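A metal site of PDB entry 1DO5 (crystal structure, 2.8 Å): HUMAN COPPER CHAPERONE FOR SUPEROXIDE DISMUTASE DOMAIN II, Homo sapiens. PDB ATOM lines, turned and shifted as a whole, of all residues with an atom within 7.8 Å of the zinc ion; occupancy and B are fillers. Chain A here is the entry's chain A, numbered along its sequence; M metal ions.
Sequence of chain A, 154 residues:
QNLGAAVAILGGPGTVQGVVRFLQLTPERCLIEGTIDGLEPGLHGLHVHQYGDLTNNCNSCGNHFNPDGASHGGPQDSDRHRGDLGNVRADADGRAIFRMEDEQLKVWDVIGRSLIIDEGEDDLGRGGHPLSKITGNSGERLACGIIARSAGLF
NE2 of His 81 sits at hydrogen-bond distance from O of Ala 70 (3.3 Å). The guanidinium group of Arg 80 lies within hydrogen-bond range of the backbone carbonyl oxygen of Asp 84 (3.3 Å). N of Gly 73 is in hydrogen-bond range of OD2 of Asp 84, 3.1 Å away. The backbone NH (N) of His 72 is in hydrogen-bond range of the backbone carbonyl oxygen (O) of Lys 133, 2.9 Å away. NE2 of His 72 sits at hydrogen-bond distance from OD1 of Asp 122, at 2.5 Å.
Residues that only touch the zinc ion: Ile 134 (3.9 Å). Within 4 Å of the zinc ion: His 64, His 72, His 81, Asp 84 and Ile 134. The nearest printed residue that does not touch the zinc ion is His 47 (4.5 Å).
The zinc ion is bound by ND1 of His 64, at 2.1 Å. The zinc ion is bound by the side-chain carboxylate (OD1) of Asp 84, 2.1 Å away. ND1 of His 72 is bound to the zinc ion (2.1 Å). ND1 of His 81 is bound to the zinc ion, 2.3 Å away.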
ATOM      1  N   LEU A  46       7.853 -18.455  16.242  1.00  0.00           N
ATOM      2  CA  LEU A  46       8.576 -18.002  15.059  1.00  0.00           C
ATOM      3  C   LEU A  46      10.024 -18.447  15.190  1.00  0.00           C
ATOM      4  O   LEU A  46      10.684 -18.125  16.167  1.00  0.00           O
ATOM      5  CB  LEU A  46       8.547 -16.470  14.959  1.00  0.00           C
ATOM      6  CG  LEU A  46       9.201 -15.920  13.694  1.00  0.00           C
ATOM      7  CD1 LEU A  46       8.428 -16.463  12.482  1.00  0.00           C
ATOM      8  CD2 LEU A  46       9.185 -14.402  13.706  1.00  0.00           C
ATOM      9  N   HIS A  47      10.526 -19.172  14.203  1.00  0.00           N
ATOM     10  CA  HIS A  47      11.906 -19.635  14.284  1.00  0.00           C
ATOM     11  C   HIS A  47      12.597 -19.578  12.937  1.00  0.00           C
ATOM     12  O   HIS A  47      11.946 -19.543  11.889  1.00  0.00           O
ATOM     13  CB  HIS A  47      11.989 -21.076  14.791  1.00  0.00           C
ATOM     14  CG  HIS A  47      11.042 -21.372  15.909  1.00  0.00           C
ATOM     15  ND1 HIS A  47       9.781 -21.900  15.686  1.00  0.00           N
ATOM     16  CD2 HIS A  47      11.130 -21.170  17.246  1.00  0.00           C
ATOM     17  CE1 HIS A  47       9.139 -21.993  16.848  1.00  0.00           C
ATOM     18  NE2 HIS A  47       9.937 -21.553  17.801  1.00  0.00           N
ATOM     19  N   VAL A  48      13.922 -19.551  12.986  1.00  0.00           N
ATOM     20  CA  VAL A  48      14.724 -19.561  11.779  1.00  0.00           C
ATOM     21  C   VAL A  48      15.225 -20.998  11.736  1.00  0.00           C
ATOM     22  O   VAL A  48      15.705 -21.518  12.745  1.00  0.00           O
ATOM     23  CB  VAL A  48      15.928 -18.617  11.896  1.00  0.00           C
ATOM     24  CG1 VAL A  48      16.823 -18.780  10.676  1.00  0.00           C
ATOM     25  CG2 VAL A  48      15.450 -17.189  12.010  1.00  0.00           C
ATOM     26  N   HIS A  49      15.060 -21.665  10.607  1.00  0.00           N
ATOM     27  CA  HIS A  49      15.535 -23.033  10.495  1.00  0.00           C
ATOM     28  C   HIS A  49      16.842 -23.062   9.735  1.00  0.00           C
ATOM     29  O   HIS A  49      17.221 -22.043   9.144  1.00  0.00           O
ATOM     30  CB  HIS A  49      14.490 -23.916   9.808  1.00  0.00           C
ATOM     31  CG  HIS A  49      13.267 -24.130  10.631  1.00  0.00           C
ATOM     32  ND1 HIS A  49      12.598 -25.338  10.676  1.00  0.00           N
ATOM     33  CD2 HIS A  49      12.584 -23.297  11.458  1.00  0.00           C
ATOM     34  CE1 HIS A  49      11.558 -25.227  11.490  1.00  0.00           C
ATOM     35  NE2 HIS A  49      11.533 -24.004  11.973  1.00  0.00           N
ATOM     36  N   ASN A  63      15.614 -28.338  10.968  1.00  0.00           N
ATOM     37  CA  ASN A  63      15.155 -27.951  12.289  1.00  0.00           C
ATOM     38  C   ASN A  63      15.526 -26.524  12.576  1.00  0.00           C
ATOM     39  O   ASN A  63      16.049 -25.827  11.712  1.00  0.00           O
ATOM     40  CB  ASN A  63      15.774 -28.875  13.341  1.00  0.00           C
ATOM     41  CG  ASN A  63      15.303 -30.301  13.195  1.00  0.00           C
ATOM     42  OD1 ASN A  63      14.119 -30.609  13.413  1.00  0.00           O
ATOM     43  ND2 ASN A  63      16.217 -31.195  12.834  1.00  0.00           N
ATOM     44  N   HIS A  64      15.246 -26.069  13.795  1.00  0.00           N
ATOM     45  CA  HIS A  64      15.589 -24.709  14.157  1.00  0.00           C
ATOM     46  C   HIS A  64      17.083 -24.529  13.943  1.00  0.00           C
ATOM     47  O   HIS A  64      17.848 -25.479  14.123  1.00  0.00           O
ATOM     48  CB  HIS A  64      15.234 -24.430  15.623  1.00  0.00           C
ATOM     49  CG  HIS A  64      13.773 -24.561  15.931  1.00  0.00           C
ATOM     50  ND1 HIS A  64      13.243 -24.291  17.177  1.00  0.00           N
ATOM     51  CD2 HIS A  64      12.728 -24.985  15.175  1.00  0.00           C
ATOM     52  CE1 HIS A  64      11.944 -24.545  17.169  1.00  0.00           C
ATOM     53  NE2 HIS A  64      11.607 -24.966  15.971  1.00  0.00           N
ATOM     54  N   PHE A  65      17.487 -23.338  13.513  1.00  0.00           N
ATOM     55  CA  PHE A  65      18.894 -22.995  13.291  1.00  0.00           C
ATOM     56  C   PHE A  65      19.515 -23.023  14.693  1.00  0.00           C
ATOM     57  O   PHE A  65      19.086 -22.288  15.575  1.00  0.00           O
ATOM     58  CB  PHE A  65      18.974 -21.607  12.655  1.00  0.00           C
ATOM     59  CG  PHE A  65      20.375 -21.115  12.481  1.00  0.00           C
ATOM     60  CD1 PHE A  65      21.289 -21.827  11.701  1.00  0.00           C
ATOM     61  CD2 PHE A  65      20.795 -19.931  13.091  1.00  0.00           C
ATOM     62  CE1 PHE A  65      22.587 -21.376  11.539  1.00  0.00           C
ATOM     63  CE2 PHE A  65      22.088 -19.468  12.944  1.00  0.00           C
ATOM     64  CZ  PHE A  65      22.992 -20.184  12.164  1.00  0.00           C
ATOM     65  N   ASN A  66      20.527 -23.866  14.886  1.00  0.00           N
ATOM     66  CA  ASN A  66      21.131 -24.036  16.213  1.00  0.00           C
ATOM     67  C   ASN A  66      22.606 -24.434  16.162  1.00  0.00           C
ATOM     68  O   ASN A  66      22.980 -25.547  16.533  1.00  0.00           O
ATOM     69  CB  ASN A  66      20.320 -25.111  16.956  1.00  0.00           C
ATOM     70  CG  ASN A  66      21.010 -25.655  18.184  1.00  0.00           C
ATOM     71  OD1 ASN A  66      21.014 -26.858  18.416  1.00  0.00           O
ATOM     72  ND2 ASN A  66      21.587 -24.765  18.983  1.00  0.00           N
ATOM     73  N   ALA A  70      22.788 -25.776  21.364  1.00  0.00           N
ATOM     74  CA  ALA A  70      22.039 -25.547  22.579  1.00  0.00           C
ATOM     75  C   ALA A  70      20.699 -26.286  22.455  1.00  0.00           C
ATOM     76  O   ALA A  70      20.465 -27.002  21.480  1.00  0.00           O
ATOM     77  CB  ALA A  70      21.792 -24.052  22.774  1.00  0.00           C
ATOM     78  N   SER A  71      19.834 -26.134  23.448  1.00  0.00           N
ATOM     79  CA  SER A  71      18.525 -26.764  23.377  1.00  0.00           C
ATOM     80  C   SER A  71      17.551 -25.613  23.111  1.00  0.00           C
ATOM     81  O   SER A  71      17.935 -24.448  23.190  1.00  0.00           O
ATOM     82  CB  SER A  71      18.198 -27.489  24.694  1.00  0.00           C
ATOM     83  OG  SER A  71      18.313 -26.644  25.815  1.00  0.00           O
ATOM     84  N   HIS A  72      16.304 -25.926  22.776  1.00  0.00           N
ATOM     85  CA  HIS A  72      15.321 -24.885  22.506  1.00  0.00           C
ATOM     86  C   HIS A  72      15.048 -24.016  23.725  1.00  0.00           C
ATOM     87  O   HIS A  72      15.136 -24.478  24.869  1.00  0.00           O
ATOM     88  CB  HIS A  72      14.005 -25.504  22.039  1.00  0.00           C
ATOM     89  CG  HIS A  72      12.960 -24.492  21.661  1.00  0.00           C
ATOM     90  ND1 HIS A  72      13.008 -23.776  20.485  1.00  0.00           N
ATOM     91  CD2 HIS A  72      11.874 -24.044  22.332  1.00  0.00           C
ATOM     92  CE1 HIS A  72      11.994 -22.939  20.448  1.00  0.00           C
ATOM     93  NE2 HIS A  72      11.286 -23.079  21.558  1.00  0.00           N
ATOM     94  N   GLY A  73      14.725 -22.742  23.480  1.00  0.00           N
ATOM     95  CA  GLY A  73      14.443 -21.818  24.552  1.00  0.00           C
ATOM     96  C   GLY A  73      13.741 -20.579  24.022  1.00  0.00           C
ATOM     97  O   GLY A  73      13.452 -20.501  22.820  1.00  0.00           O
ATOM     98  N   GLY A  74      13.458 -19.618  24.897  1.00  0.00           N
ATOM     99  CA  GLY A  74      12.823 -18.387  24.480  1.00  0.00           C
ATOM    100  C   GLY A  74      13.846 -17.445  23.874  1.00  0.00           C
ATOM    101  O   GLY A  74      15.049 -17.685  24.040  1.00  0.00           O
ATOM    102  N   ARG A  80      19.444 -21.168  24.320  1.00  0.00           N
ATOM    103  CA  ARG A  80      18.473 -21.276  23.251  1.00  0.00           C
ATOM    104  C   ARG A  80      19.130 -21.399  21.869  1.00  0.00           C
ATOM    105  O   ARG A  80      20.331 -21.217  21.711  1.00  0.00           O
ATOM    106  CB  ARG A  80      17.515 -20.069  23.298  1.00  0.00           C
ATOM    107  CG  ARG A  80      18.174 -18.696  23.188  1.00  0.00           C
ATOM    108  CD  ARG A  80      18.161 -18.194  21.748  1.00  0.00           C
ATOM    109  NE  ARG A  80      18.042 -16.737  21.666  1.00  0.00           N
ATOM    110  CZ  ARG A  80      17.955 -16.062  20.530  1.00  0.00           C
ATOM    111  NH1 ARG A  80      17.977 -16.683  19.361  1.00  0.00           N
ATOM    112  NH2 ARG A  80      17.846 -14.742  20.556  1.00  0.00           N
ATOM    113  N   HIS A  81      18.321 -21.727  20.871  1.00  0.00           N
ATOM    114  CA  HIS A  81      18.820 -21.861  19.523  1.00  0.00           C
ATOM    115  C   HIS A  81      18.992 -20.462  18.966  1.00  0.00           C
ATOM    116  O   HIS A  81      18.330 -19.531  19.415  1.00  0.00           O
ATOM    117  CB  HIS A  81      17.814 -22.647  18.684  1.00  0.00           C
ATOM    118  CG  HIS A  81      17.600 -24.045  19.156  1.00  0.00           C
ATOM    119  ND1 HIS A  81      16.488 -24.777  18.821  1.00  0.00           N
ATOM    120  CD2 HIS A  81      18.373 -24.853  19.929  1.00  0.00           C
ATOM    121  CE1 HIS A  81      16.582 -25.978  19.358  1.00  0.00           C
ATOM    122  NE2 HIS A  81      17.709 -26.052  20.039  1.00  0.00           N
ATOM    123  N   ARG A  82      19.885 -20.307  18.006  1.00  0.00           N
ATOM    124  CA  ARG A  82      20.124 -18.993  17.411  1.00  0.00           C
ATOM    125  C   ARG A  82      18.874 -18.502  16.695  1.00  0.00           C
ATOM    126  O   ARG A  82      18.588 -17.305  16.681  1.00  0.00           O
ATOM    127  CB  ARG A  82      21.311 -19.063  16.451  1.00  0.00           C
ATOM    128  CG  ARG A  82      22.612 -19.464  17.135  1.00  0.00           C
ATOM    129  CD  ARG A  82      23.407 -18.270  17.599  1.00  0.00           C
ATOM    130  NE  ARG A  82      24.315 -17.824  16.557  1.00  0.00           N
ATOM    131  CZ  ARG A  82      25.435 -18.453  16.206  1.00  0.00           C
ATOM    132  NH1 ARG A  82      25.784 -19.570  16.846  1.00  0.00           N
ATOM    133  NH2 ARG A  82      26.186 -17.995  15.221  1.00  0.00           N
ATOM    134  N   GLY A  83      18.128 -19.436  16.106  1.00  0.00           N
ATOM    135  CA  GLY A  83      16.930 -19.076  15.372  1.00  0.00           C
ATOM    136  C   GLY A  83      15.658 -18.951  16.185  1.00  0.00           C
ATOM    137  O   GLY A  83      14.590 -18.704  15.609  1.00  0.00           O
ATOM    138  N   ASP A  84      15.747 -19.098  17.496  1.00  0.00           N
ATOM    139  CA  ASP A  84      14.568 -18.990  18.330  1.00  0.00           C
ATOM    140  C   ASP A  84      14.112 -17.563  18.493  1.00  0.00           C
ATOM    141  O   ASP A  84      14.646 -16.836  19.321  1.00  0.00           O
ATOM    142  CB  ASP A  84      14.807 -19.598  19.710  1.00  0.00           C
ATOM    143  CG  ASP A  84      14.851 -21.103  19.669  1.00  0.00           C
ATOM    144  OD1 ASP A  84      14.322 -21.647  18.685  1.00  0.00           O
ATOM    145  OD2 ASP A  84      15.383 -21.723  20.604  1.00  0.00           O
ATOM    146  N   LEU A  85      13.118 -17.172  17.711  1.00  0.00           N
ATOM    147  CA  LEU A  85      12.595 -15.814  17.787  1.00  0.00           C
ATOM    148  C   LEU A  85      11.426 -15.737  18.733  1.00  0.00           C
ATOM    149  O   LEU A  85      10.848 -14.681  18.967  1.00  0.00           O
ATOM    150  CB  LEU A  85      12.208 -15.348  16.380  1.00  0.00           C
ATOM    151  CG  LEU A  85      13.455 -15.381  15.492  1.00  0.00           C
ATOM    152  CD1 LEU A  85      13.090 -14.968  14.083  1.00  0.00           C
ATOM    153  CD2 LEU A  85      14.530 -14.460  16.075  1.00  0.00           C
ATOM    154  N   GLY A  86      11.076 -16.880  19.306  1.00  0.00           N
ATOM    155  CA  GLY A  86       9.987 -16.923  20.262  1.00  0.00           C
ATOM    156  C   GLY A  86       8.619 -16.841  19.665  1.00  0.00           C
ATOM    157  O   GLY A  86       8.366 -17.370  18.577  1.00  0.00           O
ATOM    158  N   ASP A 122       4.940 -21.104  21.349  1.00  0.00           N
ATOM    159  CA  ASP A 122       6.241 -21.675  21.645  1.00  0.00           C
ATOM    160  C   ASP A 122       6.289 -21.679  23.174  1.00  0.00           C
ATOM    161  O   ASP A 122       6.211 -20.596  23.786  1.00  0.00           O
ATOM    162  CB  ASP A 122       7.324 -20.749  21.089  1.00  0.00           C
ATOM    163  CG  ASP A 122       8.719 -21.357  21.122  1.00  0.00           C
ATOM    164  OD1 ASP A 122       8.979 -22.206  22.005  1.00  0.00           O
ATOM    165  OD2 ASP A 122       9.553 -20.977  20.262  1.00  0.00           O
ATOM    166  N   GLY A 125      10.628 -23.826  25.582  1.00  0.00           N
ATOM    167  CA  GLY A 125      11.329 -24.910  26.267  1.00  0.00           C
ATOM    168  C   GLY A 125      11.030 -25.119  27.737  1.00  0.00           C
ATOM    169  O   GLY A 125      11.884 -25.617  28.466  1.00  0.00           O
ATOM    170  N   LEU A 131       9.016 -32.316  23.392  1.00  0.00           N
ATOM    171  CA  LEU A 131       9.512 -31.411  22.366  1.00  0.00           C
ATOM    172  C   LEU A 131       9.900 -30.007  22.857  1.00  0.00           C
ATOM    173  O   LEU A 131      10.481 -29.245  22.109  1.00  0.00           O
ATOM    174  CB  LEU A 131       8.490 -31.309  21.247  1.00  0.00           C
ATOM    175  CG  LEU A 131       8.159 -32.630  20.554  1.00  0.00           C
ATOM    176  CD1 LEU A 131       6.939 -32.448  19.664  1.00  0.00           C
ATOM    177  CD2 LEU A 131       9.370 -33.115  19.756  1.00  0.00           C
ATOM    178  N   SER A 132       9.571 -29.702  24.105  1.00  0.00           N
ATOM    179  CA  SER A 132       9.887 -28.391  24.678  1.00  0.00           C
ATOM    180  C   SER A 132      11.337 -27.991  24.436  1.00  0.00           C
ATOM    181  O   SER A 132      11.600 -26.929  23.888  1.00  0.00           O
ATOM    182  CB  SER A 132       9.616 -28.376  26.184  1.00  0.00           C
ATOM    183  OG  SER A 132       8.249 -28.607  26.475  1.00  0.00           O
ATOM    184  N   LYS A 133      12.273 -28.841  24.826  1.00  0.00           N
ATOM    185  CA  LYS A 133      13.691 -28.526  24.645  1.00  0.00           C
ATOM    186  C   LYS A 133      14.195 -28.777  23.223  1.00  0.00           C
ATOM    187  O   LYS A 133      15.395 -28.721  22.954  1.00  0.00           O
ATOM    188  CB  LYS A 133      14.524 -29.308  25.639  1.00  0.00           C
ATOM    189  CG  LYS A 133      14.105 -29.053  27.062  1.00  0.00           C
ATOM    190  CD  LYS A 133      14.444 -27.660  27.517  1.00  0.00           C
ATOM    191  CE  LYS A 133      14.044 -27.482  28.973  1.00  0.00           C
ATOM    192  NZ  LYS A 133      14.560 -26.245  29.586  1.00  0.00           N
ATOM    193  N   ILE A 134      13.262 -29.043  22.318  1.00  0.00           N
ATOM    194  CA  ILE A 134      13.603 -29.293  20.931  1.00  0.00           C
ATOM    195  C   ILE A 134      12.933 -28.302  19.995  1.00  0.00           C
ATOM    196  O   ILE A 134      13.606 -27.579  19.245  1.00  0.00           O
ATOM    197  CB  ILE A 134      13.191 -30.663  20.497  1.00  0.00           C
ATOM    198  CG1 ILE A 134      13.870 -31.702  21.396  1.00  0.00           C
ATOM    199  CG2 ILE A 134      13.532 -30.856  19.034  1.00  0.00           C
ATOM    200  CD1 ILE A 134      13.369 -33.078  21.195  1.00  0.00           C
ATOM    201  N   THR A 135      11.607 -28.248  20.041  1.00  0.00           N
ATOM    202  CA  THR A 135      10.838 -27.338  19.193  1.00  0.00           C
ATOM    203  C   THR A 135       9.994 -26.371  20.011  1.00  0.00           C
ATOM    204  O   THR A 135       9.363 -25.469  19.454  1.00  0.00           O
ATOM    205  CB  THR A 135       9.870 -28.106  18.270  1.00  0.00           C
ATOM    206  OG1 THR A 135       8.664 -28.409  18.983  1.00  0.00           O
ATOM    207  CG2 THR A 135      10.485 -29.406  17.808  1.00  0.00           C
ATOM    208  N   GLY A 136       9.961 -26.537  21.321  1.00  0.00           N
ATOM    209  CA  GLY A 136       9.128 -25.680  22.141  1.00  0.00           C
ATOM    210  C   GLY A 136       7.701 -26.169  21.933  1.00  0.00           C
ATOM    211  O   GLY A 136       6.755 -25.607  22.488  1.00  0.00           O
HETATM  212 ZN    ZN M   1      14.382 -23.771  18.856  1.00  0.00          ZN
